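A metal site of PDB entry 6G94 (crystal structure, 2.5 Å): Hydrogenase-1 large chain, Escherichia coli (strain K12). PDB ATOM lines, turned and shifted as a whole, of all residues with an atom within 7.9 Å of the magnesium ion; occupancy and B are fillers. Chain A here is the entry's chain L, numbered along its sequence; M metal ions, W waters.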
ATOM      1  N   PHE A  53     -12.436 -21.394   5.046  1.00  0.00           N
ATOM      2  CA  PHE A  53     -11.308 -20.470   5.057  1.00  0.00           C
ATOM      3  C   PHE A  53     -10.780 -20.334   6.466  1.00  0.00           C
ATOM      4  O   PHE A  53     -11.570 -20.228   7.394  1.00  0.00           O
ATOM      5  CB  PHE A  53     -11.734 -19.106   4.503  1.00  0.00           C
ATOM      6  CG  PHE A  53     -10.653 -18.062   4.554  1.00  0.00           C
ATOM      7  CD1 PHE A  53      -9.546 -18.139   3.697  1.00  0.00           C
ATOM      8  CD2 PHE A  53     -10.718 -17.013   5.460  1.00  0.00           C
ATOM      9  CE1 PHE A  53      -8.526 -17.207   3.760  1.00  0.00           C
ATOM     10  CE2 PHE A  53      -9.708 -16.079   5.528  1.00  0.00           C
ATOM     11  CZ  PHE A  53      -8.612 -16.167   4.673  1.00  0.00           C
ATOM     12  N   GLU A  57      -2.278 -16.828   5.808  1.00  0.00           N
ATOM     13  CA  GLU A  57      -1.508 -15.713   5.274  1.00  0.00           C
ATOM     14  C   GLU A  57      -1.639 -14.467   6.174  1.00  0.00           C
ATOM     15  O   GLU A  57      -0.723 -13.655   6.240  1.00  0.00           O
ATOM     16  CB  GLU A  57      -1.952 -15.432   3.846  1.00  0.00           C
ATOM     17  CG  GLU A  57      -1.689 -16.590   2.877  1.00  0.00           C
ATOM     18  CD  GLU A  57      -2.571 -16.556   1.647  1.00  0.00           C
ATOM     19  OE1 GLU A  57      -2.135 -17.010   0.566  1.00  0.00           O
ATOM     20  OE2 GLU A  57      -3.725 -16.059   1.745  1.00  0.00           O
ATOM     21  N   ILE A  75      -1.504 -25.941   7.281  1.00  0.00           N
ATOM     22  CA  ILE A  75      -2.413 -25.720   6.170  1.00  0.00           C
ATOM     23  C   ILE A  75      -3.126 -27.038   5.808  1.00  0.00           C
ATOM     24  O   ILE A  75      -4.329 -27.028   5.535  1.00  0.00           O
ATOM     25  CB  ILE A  75      -1.690 -25.161   4.921  1.00  0.00           C
ATOM     26  CG1 ILE A  75      -1.371 -23.686   5.124  1.00  0.00           C
ATOM     27  CG2 ILE A  75      -2.545 -25.294   3.652  1.00  0.00           C
ATOM     28  CD1 ILE A  75      -0.399 -23.138   4.094  1.00  0.00           C
ATOM     29  N   GLU A 347      -3.148 -13.921  -9.226  1.00  0.00           N
ATOM     30  CA  GLU A 347      -4.393 -14.437  -8.649  1.00  0.00           C
ATOM     31  C   GLU A 347      -5.522 -13.419  -8.793  1.00  0.00           C
ATOM     32  O   GLU A 347      -5.334 -12.230  -8.512  1.00  0.00           O
ATOM     33  CB  GLU A 347      -4.216 -14.823  -7.188  1.00  0.00           C
ATOM     34  CG  GLU A 347      -3.392 -16.075  -6.992  1.00  0.00           C
ATOM     35  CD  GLU A 347      -3.286 -16.505  -5.539  1.00  0.00           C
ATOM     36  OE1 GLU A 347      -2.607 -15.816  -4.735  1.00  0.00           O
ATOM     37  OE2 GLU A 347      -3.857 -17.569  -5.214  1.00  0.00           O
ATOM     38  N   TYR A 354     -13.059 -12.370  -1.623  1.00  0.00           N
ATOM     39  CA  TYR A 354     -11.958 -11.567  -1.154  1.00  0.00           C
ATOM     40  C   TYR A 354     -12.096 -10.162  -1.717  1.00  0.00           C
ATOM     41  O   TYR A 354     -13.026  -9.869  -2.434  1.00  0.00           O
ATOM     42  CB  TYR A 354     -10.639 -12.216  -1.559  1.00  0.00           C
ATOM     43  CG  TYR A 354     -10.412 -13.567  -0.952  1.00  0.00           C
ATOM     44  CD1 TYR A 354      -9.839 -13.697   0.293  1.00  0.00           C
ATOM     45  CD2 TYR A 354     -10.741 -14.728  -1.649  1.00  0.00           C
ATOM     46  CE1 TYR A 354      -9.619 -14.943   0.843  1.00  0.00           C
ATOM     47  CE2 TYR A 354     -10.518 -15.980  -1.110  1.00  0.00           C
ATOM     48  CZ  TYR A 354      -9.950 -16.095   0.142  1.00  0.00           C
ATOM     49  OH  TYR A 354      -9.726 -17.328   0.695  1.00  0.00           O
ATOM     50  N   PRO A 365       1.794 -12.950  -6.286  1.00  0.00           N
ATOM     51  CA  PRO A 365       1.764 -13.132  -4.839  1.00  0.00           C
ATOM     52  C   PRO A 365       2.615 -12.149  -4.039  1.00  0.00           C
ATOM     53  O   PRO A 365       2.248 -11.878  -2.908  1.00  0.00           O
ATOM     54  CB  PRO A 365       2.284 -14.562  -4.676  1.00  0.00           C
ATOM     55  CG  PRO A 365       1.896 -15.244  -5.934  1.00  0.00           C
ATOM     56  CD  PRO A 365       2.078 -14.217  -6.994  1.00  0.00           C
ATOM     57  N   ILE A 369      -2.970  -9.961  -1.841  1.00  0.00           N
ATOM     58  CA  ILE A 369      -3.818  -9.449  -0.783  1.00  0.00           C
ATOM     59  C   ILE A 369      -4.807 -10.526  -0.357  1.00  0.00           C
ATOM     60  O   ILE A 369      -5.544 -11.077  -1.192  1.00  0.00           O
ATOM     61  CB  ILE A 369      -4.600  -8.202  -1.228  1.00  0.00           C
ATOM     62  CG1 ILE A 369      -3.637  -7.111  -1.645  1.00  0.00           C
ATOM     63  CG2 ILE A 369      -5.539  -7.714  -0.138  1.00  0.00           C
ATOM     64  CD1 ILE A 369      -4.341  -5.919  -2.226  1.00  0.00           C
ATOM     65  N   THR A 370      -4.851 -10.818   0.951  1.00  0.00           N
ATOM     66  CA  THR A 370      -5.853 -11.723   1.509  1.00  0.00           C
ATOM     67  C   THR A 370      -6.751 -10.944   2.456  1.00  0.00           C
ATOM     68  O   THR A 370      -6.499 -10.860   3.660  1.00  0.00           O
ATOM     69  CB  THR A 370      -5.202 -12.893   2.244  1.00  0.00           C
ATOM     70  OG1 THR A 370      -4.216 -13.487   1.396  1.00  0.00           O
ATOM     71  CG2 THR A 370      -6.233 -13.932   2.620  1.00  0.00           C
ATOM     72  N   TRP A 397     -14.237 -19.506  -1.654  1.00  0.00           N
ATOM     73  CA  TRP A 397     -13.158 -19.038  -0.789  1.00  0.00           C
ATOM     74  C   TRP A 397     -11.802 -19.251  -1.446  1.00  0.00           C
ATOM     75  O   TRP A 397     -10.753 -18.901  -0.903  1.00  0.00           O
ATOM     76  CB  TRP A 397     -13.218 -19.703   0.589  1.00  0.00           C
ATOM     77  CG  TRP A 397     -14.294 -19.152   1.478  1.00  0.00           C
ATOM     78  CD1 TRP A 397     -15.419 -19.791   1.892  1.00  0.00           C
ATOM     79  CD2 TRP A 397     -14.337 -17.851   2.065  1.00  0.00           C
ATOM     80  NE1 TRP A 397     -16.176 -18.973   2.700  1.00  0.00           N
ATOM     81  CE2 TRP A 397     -15.532 -17.769   2.816  1.00  0.00           C
ATOM     82  CE3 TRP A 397     -13.478 -16.752   2.039  1.00  0.00           C
ATOM     83  CZ2 TRP A 397     -15.891 -16.626   3.537  1.00  0.00           C
ATOM     84  CZ3 TRP A 397     -13.843 -15.604   2.749  1.00  0.00           C
ATOM     85  CH2 TRP A 397     -15.038 -15.551   3.489  1.00  0.00           C
ATOM     86  N   LYS A 399      -9.008 -18.537  -4.298  1.00  0.00           N
ATOM     87  CA  LYS A 399      -8.568 -17.506  -5.260  1.00  0.00           C
ATOM     88  C   LYS A 399      -8.408 -18.154  -6.621  1.00  0.00           C
ATOM     89  O   LYS A 399      -8.281 -19.371  -6.702  1.00  0.00           O
ATOM     90  CB  LYS A 399      -7.252 -16.833  -4.811  1.00  0.00           C
ATOM     91  CG  LYS A 399      -7.379 -15.938  -3.590  1.00  0.00           C
ATOM     92  CD  LYS A 399      -6.041 -15.277  -3.293  1.00  0.00           C
ATOM     93  CE  LYS A 399      -6.094 -14.344  -2.075  1.00  0.00           C
ATOM     94  NZ  LYS A 399      -4.721 -13.935  -1.680  1.00  0.00           N
ATOM     95  N   PRO A 401      -5.939 -18.529  -9.461  1.00  0.00           N
ATOM     96  CA  PRO A 401      -4.600 -18.337 -10.041  1.00  0.00           C
ATOM     97  C   PRO A 401      -4.585 -18.521 -11.554  1.00  0.00           C
ATOM     98  O   PRO A 401      -5.292 -19.390 -12.076  1.00  0.00           O
ATOM     99  CB  PRO A 401      -3.755 -19.448  -9.372  1.00  0.00           C
ATOM    100  CG  PRO A 401      -4.633 -20.025  -8.305  1.00  0.00           C
ATOM    101  CD  PRO A 401      -6.048 -19.800  -8.740  1.00  0.00           C
ATOM    102  N   GLY A 513       3.686 -23.035  -4.201  1.00  0.00           N
ATOM    103  CA  GLY A 513       4.589 -21.920  -4.013  1.00  0.00           C
ATOM    104  C   GLY A 513       4.295 -21.089  -2.781  1.00  0.00           C
ATOM    105  O   GLY A 513       3.139 -20.761  -2.489  1.00  0.00           O
ATOM    106  N   TRP A 515       5.473 -17.398  -1.157  1.00  0.00           N
ATOM    107  CA  TRP A 515       6.097 -16.094  -1.404  1.00  0.00           C
ATOM    108  C   TRP A 515       6.166 -15.327  -0.087  1.00  0.00           C
ATOM    109  O   TRP A 515       5.126 -15.022   0.527  1.00  0.00           O
ATOM    110  CB  TRP A 515       5.332 -15.279  -2.466  1.00  0.00           C
ATOM    111  CG  TRP A 515       5.499 -15.742  -3.886  1.00  0.00           C
ATOM    112  CD1 TRP A 515       6.330 -15.224  -4.822  1.00  0.00           C
ATOM    113  CD2 TRP A 515       4.812 -16.834  -4.528  1.00  0.00           C
ATOM    114  NE1 TRP A 515       6.208 -15.905  -6.011  1.00  0.00           N
ATOM    115  CE2 TRP A 515       5.277 -16.896  -5.858  1.00  0.00           C
ATOM    116  CE3 TRP A 515       3.829 -17.753  -4.106  1.00  0.00           C
ATOM    117  CZ2 TRP A 515       4.807 -17.844  -6.775  1.00  0.00           C
ATOM    118  CZ3 TRP A 515       3.367 -18.675  -5.017  1.00  0.00           C
ATOM    119  CH2 TRP A 515       3.855 -18.717  -6.333  1.00  0.00           C
ATOM    120  N   TYR A 526       3.301 -12.854   3.521  1.00  0.00           N
ATOM    121  CA  TYR A 526       3.397 -14.283   3.240  1.00  0.00           C
ATOM    122  C   TYR A 526       2.184 -14.689   2.424  1.00  0.00           C
ATOM    123  O   TYR A 526       1.055 -14.694   2.919  1.00  0.00           O
ATOM    124  CB  TYR A 526       3.464 -15.092   4.543  1.00  0.00           C
ATOM    125  CG  TYR A 526       4.176 -16.421   4.420  1.00  0.00           C
ATOM    126  CD1 TYR A 526       3.528 -17.542   3.888  1.00  0.00           C
ATOM    127  CD2 TYR A 526       5.494 -16.572   4.860  1.00  0.00           C
ATOM    128  CE1 TYR A 526       4.187 -18.756   3.797  1.00  0.00           C
ATOM    129  CE2 TYR A 526       6.155 -17.795   4.773  1.00  0.00           C
ATOM    130  CZ  TYR A 526       5.497 -18.876   4.251  1.00  0.00           C
ATOM    131  OH  TYR A 526       6.174 -20.075   4.166  1.00  0.00           O
ATOM    132  N   GLN A 527       2.433 -15.039   1.163  1.00  0.00           N
ATOM    133  CA  GLN A 527       1.364 -15.470   0.258  1.00  0.00           C
ATOM    134  C   GLN A 527       1.597 -16.875  -0.297  1.00  0.00           C
ATOM    135  O   GLN A 527       2.714 -17.230  -0.719  1.00  0.00           O
ATOM    136  CB  GLN A 527       1.195 -14.474  -0.893  1.00  0.00           C
ATOM    137  CG  GLN A 527       0.577 -13.170  -0.470  1.00  0.00           C
ATOM    138  CD  GLN A 527      -0.882 -13.283  -0.152  1.00  0.00           C
ATOM    139  OE1 GLN A 527      -1.624 -13.987  -0.827  1.00  0.00           O
ATOM    140  NE2 GLN A 527      -1.318 -12.592   0.883  1.00  0.00           N
ATOM    141  N   CYS A 528       0.528 -17.679  -0.284  1.00  0.00           N
ATOM    142  CA  CYS A 528       0.595 -19.060  -0.748  1.00  0.00           C
ATOM    143  C   CYS A 528      -0.301 -19.256  -1.939  1.00  0.00           C
ATOM    144  O   CYS A 528      -1.464 -18.825  -1.942  1.00  0.00           O
ATOM    145  CB  CYS A 528       0.172 -20.017   0.372  1.00  0.00           C
ATOM    146  SG  CYS A 528       1.287 -19.981   1.783  1.00  0.00           S
ATOM    147  N   VAL A 529       0.228 -19.911  -2.962  1.00  0.00           N
ATOM    148  CA  VAL A 529      -0.577 -20.356  -4.080  1.00  0.00           C
ATOM    149  C   VAL A 529      -0.408 -21.876  -4.117  1.00  0.00           C
ATOM    150  O   VAL A 529       0.653 -22.393  -4.409  1.00  0.00           O
ATOM    151  CB  VAL A 529      -0.182 -19.674  -5.390  1.00  0.00           C
ATOM    152  CG1 VAL A 529      -1.217 -19.936  -6.470  1.00  0.00           C
ATOM    153  CG2 VAL A 529      -0.086 -18.189  -5.158  1.00  0.00           C
ATOM    154  N   VAL A 530      -1.493 -22.566  -3.804  1.00  0.00           N
ATOM    155  CA  VAL A 530      -1.460 -24.003  -3.605  1.00  0.00           C
ATOM    156  C   VAL A 530      -2.049 -24.760  -4.783  1.00  0.00           C
ATOM    157  O   VAL A 530      -2.895 -24.209  -5.480  1.00  0.00           O
ATOM    158  CB  VAL A 530      -2.163 -24.381  -2.277  1.00  0.00           C
ATOM    159  CG1 VAL A 530      -1.682 -25.716  -1.761  1.00  0.00           C
ATOM    160  CG2 VAL A 530      -1.875 -23.355  -1.211  1.00  0.00           C
ATOM    161  N   THR A 533      -5.586 -24.802  -5.367  1.00  0.00           N
ATOM    162  CA  THR A 533      -6.030 -23.449  -5.599  1.00  0.00           C
ATOM    163  C   THR A 533      -6.131 -23.308  -7.084  1.00  0.00           C
ATOM    164  O   THR A 533      -7.076 -22.729  -7.563  1.00  0.00           O
ATOM    165  CB  THR A 533      -5.115 -22.364  -5.045  1.00  0.00           C
ATOM    166  OG1 THR A 533      -4.788 -22.674  -3.697  1.00  0.00           O
ATOM    167  CG2 THR A 533      -5.826 -21.045  -5.048  1.00  0.00           C
ATOM    168  N   CYS A 579      -5.864 -27.005   1.767  1.00  0.00           N
ATOM    169  CA  CYS A 579      -4.765 -26.511   0.939  1.00  0.00           C
ATOM    170  C   CYS A 579      -5.171 -25.362   0.022  1.00  0.00           C
ATOM    171  O   CYS A 579      -4.466 -24.364  -0.085  1.00  0.00           O
ATOM    172  CB  CYS A 579      -4.183 -27.627   0.086  1.00  0.00           C
ATOM    173  SG  CYS A 579      -2.671 -28.361   0.705  1.00  0.00           S
ATOM    174  N   SER A 580      -6.308 -25.508  -0.637  1.00  0.00           N
ATOM    175  CA  SER A 580      -6.717 -24.554  -1.663  1.00  0.00           C
ATOM    176  C   SER A 580      -7.027 -23.180  -1.068  1.00  0.00           C
ATOM    177  O   SER A 580      -6.752 -22.157  -1.683  1.00  0.00           O
ATOM    178  CB  SER A 580      -7.940 -25.073  -2.432  1.00  0.00           C
ATOM    179  OG  SER A 580      -9.119 -25.013  -1.640  1.00  0.00           O
ATOM    180  N   THR A 581      -7.573 -23.182   0.152  1.00  0.00           N
ATOM    181  CA  THR A 581      -8.028 -21.937   0.782  1.00  0.00           C
ATOM    182  C   THR A 581      -7.048 -21.374   1.838  1.00  0.00           C
ATOM    183  O   THR A 581      -6.844 -20.165   1.900  1.00  0.00           O
ATOM    184  CB  THR A 581      -9.418 -22.144   1.402  1.00  0.00           C
ATOM    185  OG1 THR A 581      -9.381 -23.224   2.354  1.00  0.00           O
ATOM    186  CG2 THR A 581     -10.417 -22.507   0.320  1.00  0.00           C
ATOM    187  N   HIS A 582      -6.446 -22.263   2.637  1.00  0.00           N
ATOM    188  CA  HIS A 582      -5.496 -21.955   3.690  1.00  0.00           C
ATOM    189  C   HIS A 582      -5.896 -20.705   4.468  1.00  0.00           C
ATOM    190  O   HIS A 582      -5.088 -19.825   4.761  1.00  0.00           O
ATOM    191  CB  HIS A 582      -4.065 -21.871   3.130  1.00  0.00           C
ATOM    192  CG  HIS A 582      -3.950 -21.107   1.843  1.00  0.00           C
ATOM    193  ND1 HIS A 582      -4.214 -21.677   0.627  1.00  0.00           N
ATOM    194  CD2 HIS A 582      -3.603 -19.824   1.599  1.00  0.00           C
ATOM    195  CE1 HIS A 582      -4.037 -20.777  -0.329  1.00  0.00           C
ATOM    196  NE2 HIS A 582      -3.666 -19.647   0.240  1.00  0.00           N
ATOM    197  OXT HIS A 582      -7.068 -20.524   4.828  1.00  0.00           O
HETATM  198 MG    MG M   1      -3.078 -17.956  -0.977  1.00  0.00          MG
HETATM  199  O   HOH W   1      -4.333 -18.554  -2.420  1.00  0.00           O
HETATM  200  O   HOH W   2      -2.774 -16.309  -2.108  1.00  0.00           O
HETATM  201  O   HOH W   3      -4.820 -17.089  -0.591  1.00  0.00           O
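The side-chain carboxylate (OE2) of Glu 57 sits at hydrogen-bond distance from the side-chain hydroxyl (OG1) of Thr 370. ND1 of His 582 is in hydrogen-bond range of O of Cys 579 (2.8 Å). OE1 of Glu 57 sits close to OE1 of Gln 527. The backbone carbonyl oxygen (O) of Ser 580 sits close to a ring nitrogen (ND1) of His 582 (3.5 Å).
The nearest printed residue that does not touch the magnesium ion is Gln 527 (4.2 Å).
The magnesium ion is bound by water W3 (2.0 Å), water W1 (2.0 Å), water W2 (2.0 Å), OE1 of Glu 57 (2.0 Å), O of Cys 528 (2.1 Å) and NE2 of His 582 (2.2 Å).
Water W2 lies within hydrogen-bond range of the side-chain carboxylate (OE1) of Glu 347 (2.7 Å), the side-chain amide oxygen (OE1) of Gln 527 (2.9 Å) and the side-chain amino group (NZ) of Lys 399 (3.1 Å). Water W3 lies within hydrogen-bond range of OE2 of Glu 57 (2.8 Å) and NZ of Lys 399 (3.3 Å).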
